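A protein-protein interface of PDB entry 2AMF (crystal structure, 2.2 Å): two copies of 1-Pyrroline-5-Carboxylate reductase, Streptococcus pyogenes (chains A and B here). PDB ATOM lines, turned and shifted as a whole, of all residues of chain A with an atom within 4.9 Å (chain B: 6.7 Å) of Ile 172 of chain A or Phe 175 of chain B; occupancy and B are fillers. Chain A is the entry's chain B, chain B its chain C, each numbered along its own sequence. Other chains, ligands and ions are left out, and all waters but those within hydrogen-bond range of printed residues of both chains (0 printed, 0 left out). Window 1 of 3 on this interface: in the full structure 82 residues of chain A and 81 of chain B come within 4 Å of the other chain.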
ATOM      1  N   SER A 168      23.863  17.716  38.430  1.00  0.00           N
ATOM      2  CA  SER A 168      23.573  17.561  37.003  1.00  0.00           C
ATOM      3  C   SER A 168      22.450  16.596  36.622  1.00  0.00           C
ATOM      4  O   SER A 168      21.854  16.773  35.564  1.00  0.00           O
ATOM      5  CB  SER A 168      24.845  17.245  36.214  1.00  0.00           C
ATOM      6  OG  SER A 168      25.334  15.962  36.549  1.00  0.00           O
ATOM      7  N   PRO A 169      22.140  15.573  37.461  1.00  0.00           N
ATOM      8  CA  PRO A 169      20.993  14.746  37.062  1.00  0.00           C
ATOM      9  C   PRO A 169      19.758  15.606  36.801  1.00  0.00           C
ATOM     10  O   PRO A 169      19.022  15.354  35.869  1.00  0.00           O
ATOM     11  CB  PRO A 169      20.760  13.852  38.285  1.00  0.00           C
ATOM     12  CG  PRO A 169      22.135  13.723  38.900  1.00  0.00           C
ATOM     13  CD  PRO A 169      22.743  15.088  38.728  1.00  0.00           C
ATOM     14  N   ALA A 170      19.568  16.628  37.619  1.00  0.00           N
ATOM     15  CA  ALA A 170      18.451  17.568  37.474  1.00  0.00           C
ATOM     16  C   ALA A 170      18.524  18.321  36.136  1.00  0.00           C
ATOM     17  O   ALA A 170      17.487  18.589  35.514  1.00  0.00           O
ATOM     18  CB  ALA A 170      18.485  18.558  38.625  1.00  0.00           C
ATOM     19  N   TYR A 171      19.753  18.661  35.703  1.00  0.00           N
ATOM     20  CA  TYR A 171      19.959  19.461  34.485  1.00  0.00           C
ATOM     21  C   TYR A 171      19.751  18.559  33.291  1.00  0.00           C
ATOM     22  O   TYR A 171      19.160  18.966  32.282  1.00  0.00           O
ATOM     23  CB  TYR A 171      21.351  20.151  34.461  1.00  0.00           C
ATOM     24  CG  TYR A 171      21.727  20.912  35.746  1.00  0.00           C
ATOM     25  CD1 TYR A 171      20.745  21.501  36.566  1.00  0.00           C
ATOM     26  CD2 TYR A 171      23.065  21.052  36.138  1.00  0.00           C
ATOM     27  CE1 TYR A 171      21.088  22.198  37.743  1.00  0.00           C
ATOM     28  CE2 TYR A 171      23.417  21.738  37.312  1.00  0.00           C
ATOM     29  CZ  TYR A 171      22.422  22.314  38.103  1.00  0.00           C
ATOM     30  OH  TYR A 171      22.749  22.976  39.277  1.00  0.00           O
ATOM     31  N   ILE A 172      20.222  17.321  33.420  1.00  0.00           N
ATOM     32  CA  ILE A 172      19.946  16.272  32.460  1.00  0.00           C
ATOM     33  C   ILE A 172      18.433  16.061  32.294  1.00  0.00           C
ATOM     34  O   ILE A 172      17.932  15.978  31.173  1.00  0.00           O
ATOM     35  CB  ILE A 172      20.655  14.924  32.853  1.00  0.00           C
ATOM     36  CG1 ILE A 172      22.183  15.048  32.719  1.00  0.00           C
ATOM     37  CG2 ILE A 172      20.176  13.802  31.971  1.00  0.00           C
ATOM     38  CD1 ILE A 172      22.948  14.239  33.743  1.00  0.00           C
ATOM     39  N   TYR A 173      17.702  15.992  33.405  1.00  0.00           N
ATOM     40  CA  TYR A 173      16.240  15.857  33.328  1.00  0.00           C
ATOM     41  C   TYR A 173      15.570  17.036  32.626  1.00  0.00           C
ATOM     42  O   TYR A 173      14.663  16.826  31.831  1.00  0.00           O
ATOM     43  CB  TYR A 173      15.598  15.571  34.712  1.00  0.00           C
ATOM     44  CG  TYR A 173      16.023  14.245  35.297  1.00  0.00           C
ATOM     45  CD1 TYR A 173      15.986  13.078  34.527  1.00  0.00           C
ATOM     46  CD2 TYR A 173      16.491  14.152  36.608  1.00  0.00           C
ATOM     47  CE1 TYR A 173      16.397  11.858  35.035  1.00  0.00           C
ATOM     48  CE2 TYR A 173      16.909  12.916  37.138  1.00  0.00           C
ATOM     49  CZ  TYR A 173      16.853  11.780  36.348  1.00  0.00           C
ATOM     50  OH  TYR A 173      17.251  10.553  36.854  1.00  0.00           O
ATOM     51  N   LEU A 174      16.010  18.267  32.915  1.00  0.00           N
ATOM     52  CA  LEU A 174      15.395  19.473  32.309  1.00  0.00           C
ATOM     53  C   LEU A 174      15.554  19.485  30.789  1.00  0.00           C
ATOM     54  O   LEU A 174      14.605  19.823  30.052  1.00  0.00           O
ATOM     55  CB  LEU A 174      15.960  20.752  32.924  1.00  0.00           C
ATOM     56  CG  LEU A 174      15.267  22.075  32.539  1.00  0.00           C
ATOM     57  CD1 LEU A 174      13.879  22.217  33.178  1.00  0.00           C
ATOM     58  CD2 LEU A 174      16.109  23.304  32.866  1.00  0.00           C
ATOM     59  N   PHE A 175      16.746  19.091  30.341  1.00  0.00           N
ATOM     60  CA  PHE A 175      17.089  18.899  28.944  1.00  0.00           C
ATOM     61  C   PHE A 175      16.209  17.833  28.289  1.00  0.00           C
ATOM     62  O   PHE A 175      15.615  18.067  27.234  1.00  0.00           O
ATOM     63  CB  PHE A 175      18.576  18.483  28.847  1.00  0.00           C
ATOM     64  CG  PHE A 175      19.091  18.316  27.421  1.00  0.00           C
ATOM     65  CD1 PHE A 175      19.323  19.426  26.606  1.00  0.00           C
ATOM     66  CD2 PHE A 175      19.358  17.045  26.908  1.00  0.00           C
ATOM     67  CE1 PHE A 175      19.803  19.268  25.295  1.00  0.00           C
ATOM     68  CE2 PHE A 175      19.852  16.874  25.607  1.00  0.00           C
ATOM     69  CZ  PHE A 175      20.071  17.990  24.800  1.00  0.00           C
ATOM     70  N   ILE A 176      16.154  16.653  28.908  1.00  0.00           N
ATOM     71  CA  ILE A 176      15.270  15.572  28.445  1.00  0.00           C
ATOM     72  C   ILE A 176      13.807  16.055  28.391  1.00  0.00           C
ATOM     73  O   ILE A 176      13.093  15.814  27.416  1.00  0.00           O
ATOM     74  CB  ILE A 176      15.395  14.296  29.337  1.00  0.00           C
ATOM     75  CG1 ILE A 176      16.744  13.609  29.097  1.00  0.00           C
ATOM     76  CG2 ILE A 176      14.223  13.312  29.056  1.00  0.00           C
ATOM     77  CD1 ILE A 176      17.059  12.395  30.037  1.00  0.00           C
ATOM     78  N   LEU A 241      23.364  27.466  23.885  1.00  0.00           N
ATOM     79  CA  LEU A 241      23.298  26.222  24.699  1.00  0.00           C
ATOM     80  C   LEU A 241      24.510  25.979  25.624  1.00  0.00           C
ATOM     81  O   LEU A 241      24.342  25.718  26.812  1.00  0.00           O
ATOM     82  CB  LEU A 241      23.082  24.968  23.839  1.00  0.00           C
ATOM     83  CG  LEU A 241      23.065  23.771  24.817  1.00  0.00           C
ATOM     84  CD1 LEU A 241      21.650  23.440  25.319  1.00  0.00           C
ATOM     85  CD2 LEU A 241      23.781  22.550  24.349  1.00  0.00           C
ATOM     86  N   VAL A 245      24.702  26.249  29.828  1.00  0.00           N
ATOM     87  CA  VAL A 245      25.080  25.121  30.677  1.00  0.00           C
ATOM     88  C   VAL A 245      26.287  25.485  31.544  1.00  0.00           C
ATOM     89  O   VAL A 245      26.289  25.235  32.756  1.00  0.00           O
ATOM     90  CB  VAL A 245      25.375  23.863  29.831  1.00  0.00           C
ATOM     91  CG1 VAL A 245      25.881  22.714  30.711  1.00  0.00           C
ATOM     92  CG2 VAL A 245      24.104  23.424  29.093  1.00  0.00           C
ATOM     93  N   ALA B 170      23.363  14.408  18.430  1.00  0.00           N
ATOM     94  CA  ALA B 170      24.268  15.574  18.337  1.00  0.00           C
ATOM     95  C   ALA B 170      23.984  16.620  19.395  1.00  0.00           C
ATOM     96  O   ALA B 170      24.904  17.270  19.884  1.00  0.00           O
ATOM     97  CB  ALA B 170      24.164  16.212  16.956  1.00  0.00           C
ATOM     98  N   TYR B 171      22.707  16.816  19.727  1.00  0.00           N
ATOM     99  CA  TYR B 171      22.339  17.833  20.719  1.00  0.00           C
ATOM    100  C   TYR B 171      22.690  17.360  22.129  1.00  0.00           C
ATOM    101  O   TYR B 171      23.156  18.144  22.983  1.00  0.00           O
ATOM    102  CB  TYR B 171      20.861  18.241  20.591  1.00  0.00           C
ATOM    103  CG  TYR B 171      20.405  18.530  19.158  1.00  0.00           C
ATOM    104  CD1 TYR B 171      21.289  19.059  18.197  1.00  0.00           C
ATOM    105  CD2 TYR B 171      19.086  18.316  18.775  1.00  0.00           C
ATOM    106  CE1 TYR B 171      20.869  19.333  16.885  1.00  0.00           C
ATOM    107  CE2 TYR B 171      18.663  18.576  17.467  1.00  0.00           C
ATOM    108  CZ  TYR B 171      19.562  19.086  16.525  1.00  0.00           C
ATOM    109  OH  TYR B 171      19.129  19.334  15.222  1.00  0.00           O
ATOM    110  N   ILE B 172      22.479  16.061  22.353  1.00  0.00           N
ATOM    111  CA  ILE B 172      22.878  15.378  23.569  1.00  0.00           C
ATOM    112  C   ILE B 172      24.386  15.440  23.715  1.00  0.00           C
ATOM    113  O   ILE B 172      24.897  15.704  24.805  1.00  0.00           O
ATOM    114  CB  ILE B 172      22.395  13.901  23.532  1.00  0.00           C
ATOM    115  CG1 ILE B 172      20.861  13.830  23.664  1.00  0.00           C
ATOM    116  CG2 ILE B 172      23.090  13.043  24.610  1.00  0.00           C
ATOM    117  CD1 ILE B 172      20.241  12.587  22.942  1.00  0.00           C
ATOM    118  N   TYR B 173      25.106  15.213  22.621  1.00  0.00           N
ATOM    119  CA  TYR B 173      26.559  15.341  22.652  1.00  0.00           C
ATOM    120  C   TYR B 173      27.040  16.763  22.977  1.00  0.00           C
ATOM    121  O   TYR B 173      27.916  16.949  23.832  1.00  0.00           O
ATOM    122  CB  TYR B 173      27.207  14.772  21.384  1.00  0.00           C
ATOM    123  CG  TYR B 173      27.049  13.257  21.254  1.00  0.00           C
ATOM    124  CD1 TYR B 173      27.262  12.412  22.349  1.00  0.00           C
ATOM    125  CD2 TYR B 173      26.681  12.667  20.034  1.00  0.00           C
ATOM    126  CE1 TYR B 173      27.108  11.018  22.235  1.00  0.00           C
ATOM    127  CE2 TYR B 173      26.506  11.285  19.917  1.00  0.00           C
ATOM    128  CZ  TYR B 173      26.724  10.464  21.019  1.00  0.00           C
ATOM    129  OH  TYR B 173      26.575   9.081  20.908  1.00  0.00           O
ATOM    130  N   LEU B 174      26.450  17.768  22.325  1.00  0.00           N
ATOM    131  CA  LEU B 174      26.770  19.163  22.670  1.00  0.00           C
ATOM    132  C   LEU B 174      26.563  19.486  24.159  1.00  0.00           C
ATOM    133  O   LEU B 174      27.338  20.232  24.769  1.00  0.00           O
ATOM    134  CB  LEU B 174      25.977  20.151  21.802  1.00  0.00           C
ATOM    135  CG  LEU B 174      26.539  21.586  21.760  1.00  0.00           C
ATOM    136  CD1 LEU B 174      27.877  21.615  21.018  1.00  0.00           C
ATOM    137  CD2 LEU B 174      25.535  22.564  21.131  1.00  0.00           C
ATOM    138  N   PHE B 175      25.513  18.910  24.728  1.00  0.00           N
ATOM    139  CA  PHE B 175      25.134  19.178  26.100  1.00  0.00           C
ATOM    140  C   PHE B 175      26.126  18.506  27.044  1.00  0.00           C
ATOM    141  O   PHE B 175      26.641  19.131  27.963  1.00  0.00           O
ATOM    142  CB  PHE B 175      23.690  18.677  26.310  1.00  0.00           C
ATOM    143  CG  PHE B 175      23.203  18.771  27.718  1.00  0.00           C
ATOM    144  CD1 PHE B 175      22.745  19.987  28.234  1.00  0.00           C
ATOM    145  CD2 PHE B 175      23.160  17.627  28.526  1.00  0.00           C
ATOM    146  CE1 PHE B 175      22.264  20.057  29.552  1.00  0.00           C
ATOM    147  CE2 PHE B 175      22.670  17.693  29.819  1.00  0.00           C
ATOM    148  CZ  PHE B 175      22.230  18.917  30.337  1.00  0.00           C
ATOM    149  N   ILE B 176      26.421  17.235  26.772  1.00  0.00           N
ATOM    150  CA  ILE B 176      27.479  16.520  27.466  1.00  0.00           C
ATOM    151  C   ILE B 176      28.825  17.272  27.390  1.00  0.00           C
ATOM    152  O   ILE B 176      29.499  17.474  28.421  1.00  0.00           O
ATOM    153  CB  ILE B 176      27.614  15.063  26.945  1.00  0.00           C
ATOM    154  CG1 ILE B 176      26.433  14.210  27.440  1.00  0.00           C
ATOM    155  CG2 ILE B 176      28.909  14.435  27.407  1.00  0.00           C
ATOM    156  CD1 ILE B 176      26.310  12.832  26.761  1.00  0.00           C
ATOM    157  N   GLU B 177      29.197  17.689  26.183  1.00  0.00           N
ATOM    158  CA  GLU B 177      30.434  18.421  25.961  1.00  0.00           C
ATOM    159  C   GLU B 177      30.445  19.708  26.784  1.00  0.00           C
ATOM    160  O   GLU B 177      31.488  20.071  27.354  1.00  0.00           O
ATOM    161  CB  GLU B 177      30.586  18.758  24.474  1.00  0.00           C
ATOM    162  CG  GLU B 177      31.779  19.657  24.133  1.00  0.00           C
ATOM    163  CD  GLU B 177      33.108  18.959  24.291  1.00  0.00           C
ATOM    164  OE1 GLU B 177      33.120  17.740  24.544  1.00  0.00           O
ATOM    165  OE2 GLU B 177      34.159  19.629  24.152  1.00  0.00           O
ATOM    166  N   ALA B 178      29.284  20.373  26.851  1.00  0.00           N
ATOM    167  CA  ALA B 178      29.145  21.611  27.597  1.00  0.00           C
ATOM    168  C   ALA B 178      29.360  21.394  29.099  1.00  0.00           C
ATOM    169  O   ALA B 178      29.996  22.217  29.764  1.00  0.00           O
ATOM    170  CB  ALA B 178      27.796  22.262  27.303  1.00  0.00           C
ATOM    171  N   LEU B 179      28.861  20.272  29.626  1.00  0.00           N
ATOM    172  CA  LEU B 179      29.076  19.945  31.037  1.00  0.00           C
ATOM    173  C   LEU B 179      30.561  19.710  31.288  1.00  0.00           C
ATOM    174  O   LEU B 179      31.120  20.229  32.260  1.00  0.00           O
ATOM    175  CB  LEU B 179      28.242  18.723  31.461  1.00  0.00           C
ATOM    176  CG  LEU B 179      26.739  19.006  31.620  1.00  0.00           C
ATOM    177  CD1 LEU B 179      25.873  17.741  31.638  1.00  0.00           C
ATOM    178  CD2 LEU B 179      26.498  19.859  32.844  1.00  0.00           C
ATOM    179  N   ALA B 180      31.201  18.940  30.409  1.00  0.00           N
ATOM    180  CA  ALA B 180      32.618  18.629  30.558  1.00  0.00           C
ATOM    181  C   ALA B 180      33.507  19.877  30.463  1.00  0.00           C
ATOM    182  O   ALA B 180      34.445  20.054  31.245  1.00  0.00           O
ATOM    183  CB  ALA B 180      33.045  17.561  29.552  1.00  0.00           C
ATOM    184  N   VAL B 197      30.402  12.872  33.657  1.00  0.00           N
ATOM    185  CA  VAL B 197      29.062  13.259  33.215  1.00  0.00           C
ATOM    186  C   VAL B 197      28.391  12.201  32.337  1.00  0.00           C
ATOM    187  O   VAL B 197      27.187  12.010  32.427  1.00  0.00           O
ATOM    188  CB  VAL B 197      28.924  14.745  32.653  1.00  0.00           C
ATOM    189  CG1 VAL B 197      30.096  15.631  33.080  1.00  0.00           C
ATOM    190  CG2 VAL B 197      28.665  14.779  31.165  1.00  0.00           C
ATOM    191  N   THR B 200      26.962   9.758  34.685  1.00  0.00           N
ATOM    192  CA  THR B 200      25.808  10.359  35.319  1.00  0.00           C
ATOM    193  C   THR B 200      24.616  10.437  34.341  1.00  0.00           C
ATOM    194  O   THR B 200      23.472  10.156  34.728  1.00  0.00           O
ATOM    195  CB  THR B 200      26.153  11.751  35.909  1.00  0.00           C
ATOM    196  OG1 THR B 200      27.293  11.638  36.760  1.00  0.00           O
ATOM    197  CG2 THR B 200      24.988  12.314  36.705  1.00  0.00           C
ATOM    198  N   VAL B 201      24.877  10.811  33.086  1.00  0.00           N
ATOM    199  CA  VAL B 201      23.831  10.828  32.049  1.00  0.00           C
ATOM    200  C   VAL B 201      23.225   9.436  31.873  1.00  0.00           C
ATOM    201  O   VAL B 201      22.010   9.259  31.930  1.00  0.00           O
ATOM    202  CB  VAL B 201      24.364  11.352  30.684  1.00  0.00           C
ATOM    203  CG1 VAL B 201      23.361  11.078  29.571  1.00  0.00           C
ATOM    204  CG2 VAL B 201      24.681  12.842  30.753  1.00  0.00           C
ATOM    205  N   LEU B 202      24.085   8.444  31.666  1.00  0.00           N
ATOM    206  CA  LEU B 202      23.660   7.044  31.591  1.00  0.00           C
ATOM    207  C   LEU B 202      22.719   6.645  32.740  1.00  0.00           C
ATOM    208  O   LEU B 202      21.616   6.118  32.503  1.00  0.00           O
ATOM    209  CB  LEU B 202      24.889   6.135  31.608  1.00  0.00           C
ATOM    210  CG  LEU B 202      25.311   5.281  30.413  1.00  0.00           C
ATOM    211  CD1 LEU B 202      24.610   5.633  29.130  1.00  0.00           C
ATOM    212  CD2 LEU B 202      26.844   5.306  30.252  1.00  0.00           C
ATOM    213  N   SER B 204      21.133   8.532  35.072  1.00  0.00           N
ATOM    214  CA  SER B 204      19.935   9.372  35.167  1.00  0.00           C
ATOM    215  C   SER B 204      18.867   8.919  34.165  1.00  0.00           C
ATOM    216  O   SER B 204      17.696   8.783  34.524  1.00  0.00           O
ATOM    217  CB  SER B 204      20.266  10.858  34.895  1.00  0.00           C
ATOM    218  OG  SER B 204      21.147  11.360  35.865  1.00  0.00           O
ATOM    219  N   ALA B 205      19.267   8.717  32.913  1.00  0.00           N
ATOM    220  CA  ALA B 205      18.318   8.259  31.892  1.00  0.00           C
ATOM    221  C   ALA B 205      17.768   6.853  32.250  1.00  0.00           C
ATOM    222  O   ALA B 205      16.579   6.549  32.071  1.00  0.00           O
ATOM    223  CB  ALA B 205      18.974   8.273  30.517  1.00  0.00           C
ATOM    224  N   PRO B 215      10.383  13.480  34.708  1.00  0.00           N
ATOM    225  CA  PRO B 215      11.635  14.270  34.870  1.00  0.00           C
ATOM    226  C   PRO B 215      11.524  15.405  35.895  1.00  0.00           C
ATOM    227  O   PRO B 215      12.447  15.632  36.676  1.00  0.00           O
ATOM    228  CB  PRO B 215      11.877  14.850  33.476  1.00  0.00           C
ATOM    229  CG  PRO B 215      11.141  13.915  32.535  1.00  0.00           C
ATOM    230  CD  PRO B 215       9.974  13.332  33.296  1.00  0.00           C
ATOM    231  N   ILE B 219      13.472  16.338  39.404  1.00  0.00           N
ATOM    232  CA  ILE B 219      14.057  17.657  39.629  1.00  0.00           C
ATOM    233  C   ILE B 219      13.703  18.122  41.028  1.00  0.00           C
ATOM    234  O   ILE B 219      14.572  18.590  41.774  1.00  0.00           O
ATOM    235  CB  ILE B 219      13.641  18.680  38.537  1.00  0.00           C
ATOM    236  CG1 ILE B 219      14.297  18.313  37.194  1.00  0.00           C
ATOM    237  CG2 ILE B 219      14.013  20.106  38.963  1.00  0.00           C
ATOM    238  CD1 ILE B 219      13.734  19.051  35.971  1.00  0.00           C
ATOM    239  N   LEU B 236      19.675  28.074  34.496  1.00  0.00           N
ATOM    240  CA  LEU B 236      19.218  27.457  33.243  1.00  0.00           C
ATOM    241  C   LEU B 236      17.943  28.111  32.749  1.00  0.00           C
ATOM    242  O   LEU B 236      17.805  28.385  31.561  1.00  0.00           O
ATOM    243  CB  LEU B 236      18.981  25.943  33.418  1.00  0.00           C
ATOM    244  CG  LEU B 236      20.203  25.027  33.536  1.00  0.00           C
ATOM    245  CD1 LEU B 236      19.796  23.567  33.890  1.00  0.00           C
ATOM    246  CD2 LEU B 236      21.111  25.068  32.297  1.00  0.00           C
ATOM    247  N   LEU B 241      17.372  27.514  28.841  1.00  0.00           N
ATOM    248  CA  LEU B 241      17.677  26.160  28.372  1.00  0.00           C
ATOM    249  C   LEU B 241      16.526  25.496  27.566  1.00  0.00           C
ATOM    250  O   LEU B 241      16.733  25.009  26.453  1.00  0.00           O
ATOM    251  CB  LEU B 241      18.125  25.225  29.507  1.00  0.00           C
ATOM    252  CG  LEU B 241      18.401  23.849  28.862  1.00  0.00           C
ATOM    253  CD1 LEU B 241      19.853  23.648  28.498  1.00  0.00           C
ATOM    254  CD2 LEU B 241      17.876  22.683  29.624  1.00  0.00           C
ATOM    255  N   VAL B 245      16.503  24.576  23.455  1.00  0.00           N
ATOM    256  CA  VAL B 245      16.333  23.219  22.932  1.00  0.00           C
ATOM    257  C   VAL B 245      15.101  23.147  22.014  1.00  0.00           C
ATOM    258  O   VAL B 245      15.163  22.602  20.911  1.00  0.00           O
ATOM    259  CB  VAL B 245      16.252  22.209  24.107  1.00  0.00           C
ATOM    260  CG1 VAL B 245      15.909  20.768  23.626  1.00  0.00           C
ATOM    261  CG2 VAL B 245      17.577  22.221  24.882  1.00  0.00           C
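The side-chain hydroxyl (OH) of Tyr 173 of chain A lies within hydrogen-bond range of the backbone carbonyl oxygen (O) of Ser 204 of chain B, 3.0 Å away.
OG of Ser 204 of chain B sits at hydrogen-bond distance from O of Thr 200 of chain B, 2.9 Å away.
The backbone NH of Leu 241 of chain B lies within hydrogen-bond range of the backbone carbonyl oxygen of Leu 236 of chain B, at 2.9 Å.
Among the printed residues, pairs that only touch across the chains: Pro 169 of chain A with Ser 204 of chain B (3.5 Å), Tyr 171 of chain A with Leu 236 of chain B (3.5 Å), Phe 175 of chain A with Tyr 171 of chain B (3.6 Å), Ala 170 of chain A with Ile 219 of chain B (3.6 Å), Val 245 of chain A with Leu 179 of chain B (3.6 Å), Tyr 171 of chain A with Phe 175 of chain B (3.6 Å), Leu 241 of chain A with Leu 241 of chain B (3.7 Å), Leu 241 of chain A with Leu 174 of chain B (3.7 Å), Ser 168 of chain A with Thr 200 of chain B (3.7 Å), Tyr 173 of chain A with Pro 215 of chain B (3.7 Å), Phe 175 of chain A with Val 245 of chain B (3.7 Å), Ile 172 of chain A with Val 201 of chain B (3.7 Å), Leu 174 of chain A with Leu 241 of chain B (3.7 Å), Phe 175 of chain A with Ile 172 of chain B (3.7 Å), Val 245 of chain A with Phe 175 of chain B (3.8 Å), Phe 175 of chain A with Phe 175 of chain B (3.8 Å), Phe 175 of chain A with Leu 241 of chain B (3.8 Å), Leu 174 of chain A with Leu 236 of chain B (3.8 Å), Val 245 of chain A with Ala 178 of chain B (3.8 Å), Pro 169 of chain A with Thr 200 of chain B (3.9 Å), Leu 174 of chain A with Ile 219 of chain B (3.9 Å), Tyr 173 of chain A with Ile 219 of chain B (3.9 Å) and Ile 172 of chain A with Phe 175 of chain B (3.96 Å).
Of the printed residues of chain B, Ile 172 of chain A touches Phe 175 (3.96 Å) and Val 201 (3.7 Å).
Of chain A, only Tyr 171, Ile 172, Phe 175 and Val 245 come within 4 Å of Phe 175 of chain B.
Printed residues of chain A within 4 Å of Thr 200 of chain B: Ser 168 and Pro 169.
Printed residues of chain A within 4 Å of Ser 204 of chain B: Pro 169 (3.5 Å) and Tyr 173 (3.0 Å).
Of the printed residues of chain A, Leu 236 of chain B touches Tyr 171 and Leu 174.
Printed residues of chain A within 4 Å of Leu 241 of chain B: Leu 174 (3.7 Å), Phe 175 (3.8 Å) and Leu 241 (3.7 Å).
The nearest printed residue of chain B that does not touch Ile 172 of chain A is Ser 204 of chain B (4.004 Å).
The nearest residue of chain A that does not touch Phe 175 of chain B is Leu 241 of chain A (4.03 Å).
Of the 11 printed residues of chain A, 10 touch a printed residue of chain B.
Of the 22 printed residues of chain B, 14 touch a printed residue of chain A.
Among the printed residues, 24 pairs touch across the chains.
Ile 172 of chain A touches Phe 175 of chain B, and with the chains exchanged Phe 175 of chain A touches Ile 172 of chain B.
Phe 175 of chain A touches its own counterpart, Phe 175 of chain B.
Phe 175 of chain A touches Val 245 of chain B, and with the chains exchanged Val 245 of chain A touches Phe 175 of chain B.
Leu 241 of chain A touches its own counterpart, Leu 241 of chain B.
Positions printed for both chains: 170, 171, 172, 173, 174, 175, 176, 241 and 245.
Of the 24 pairs that touch across the chains among the printed residues, 10 have their exchanged pair printed and touching as well.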
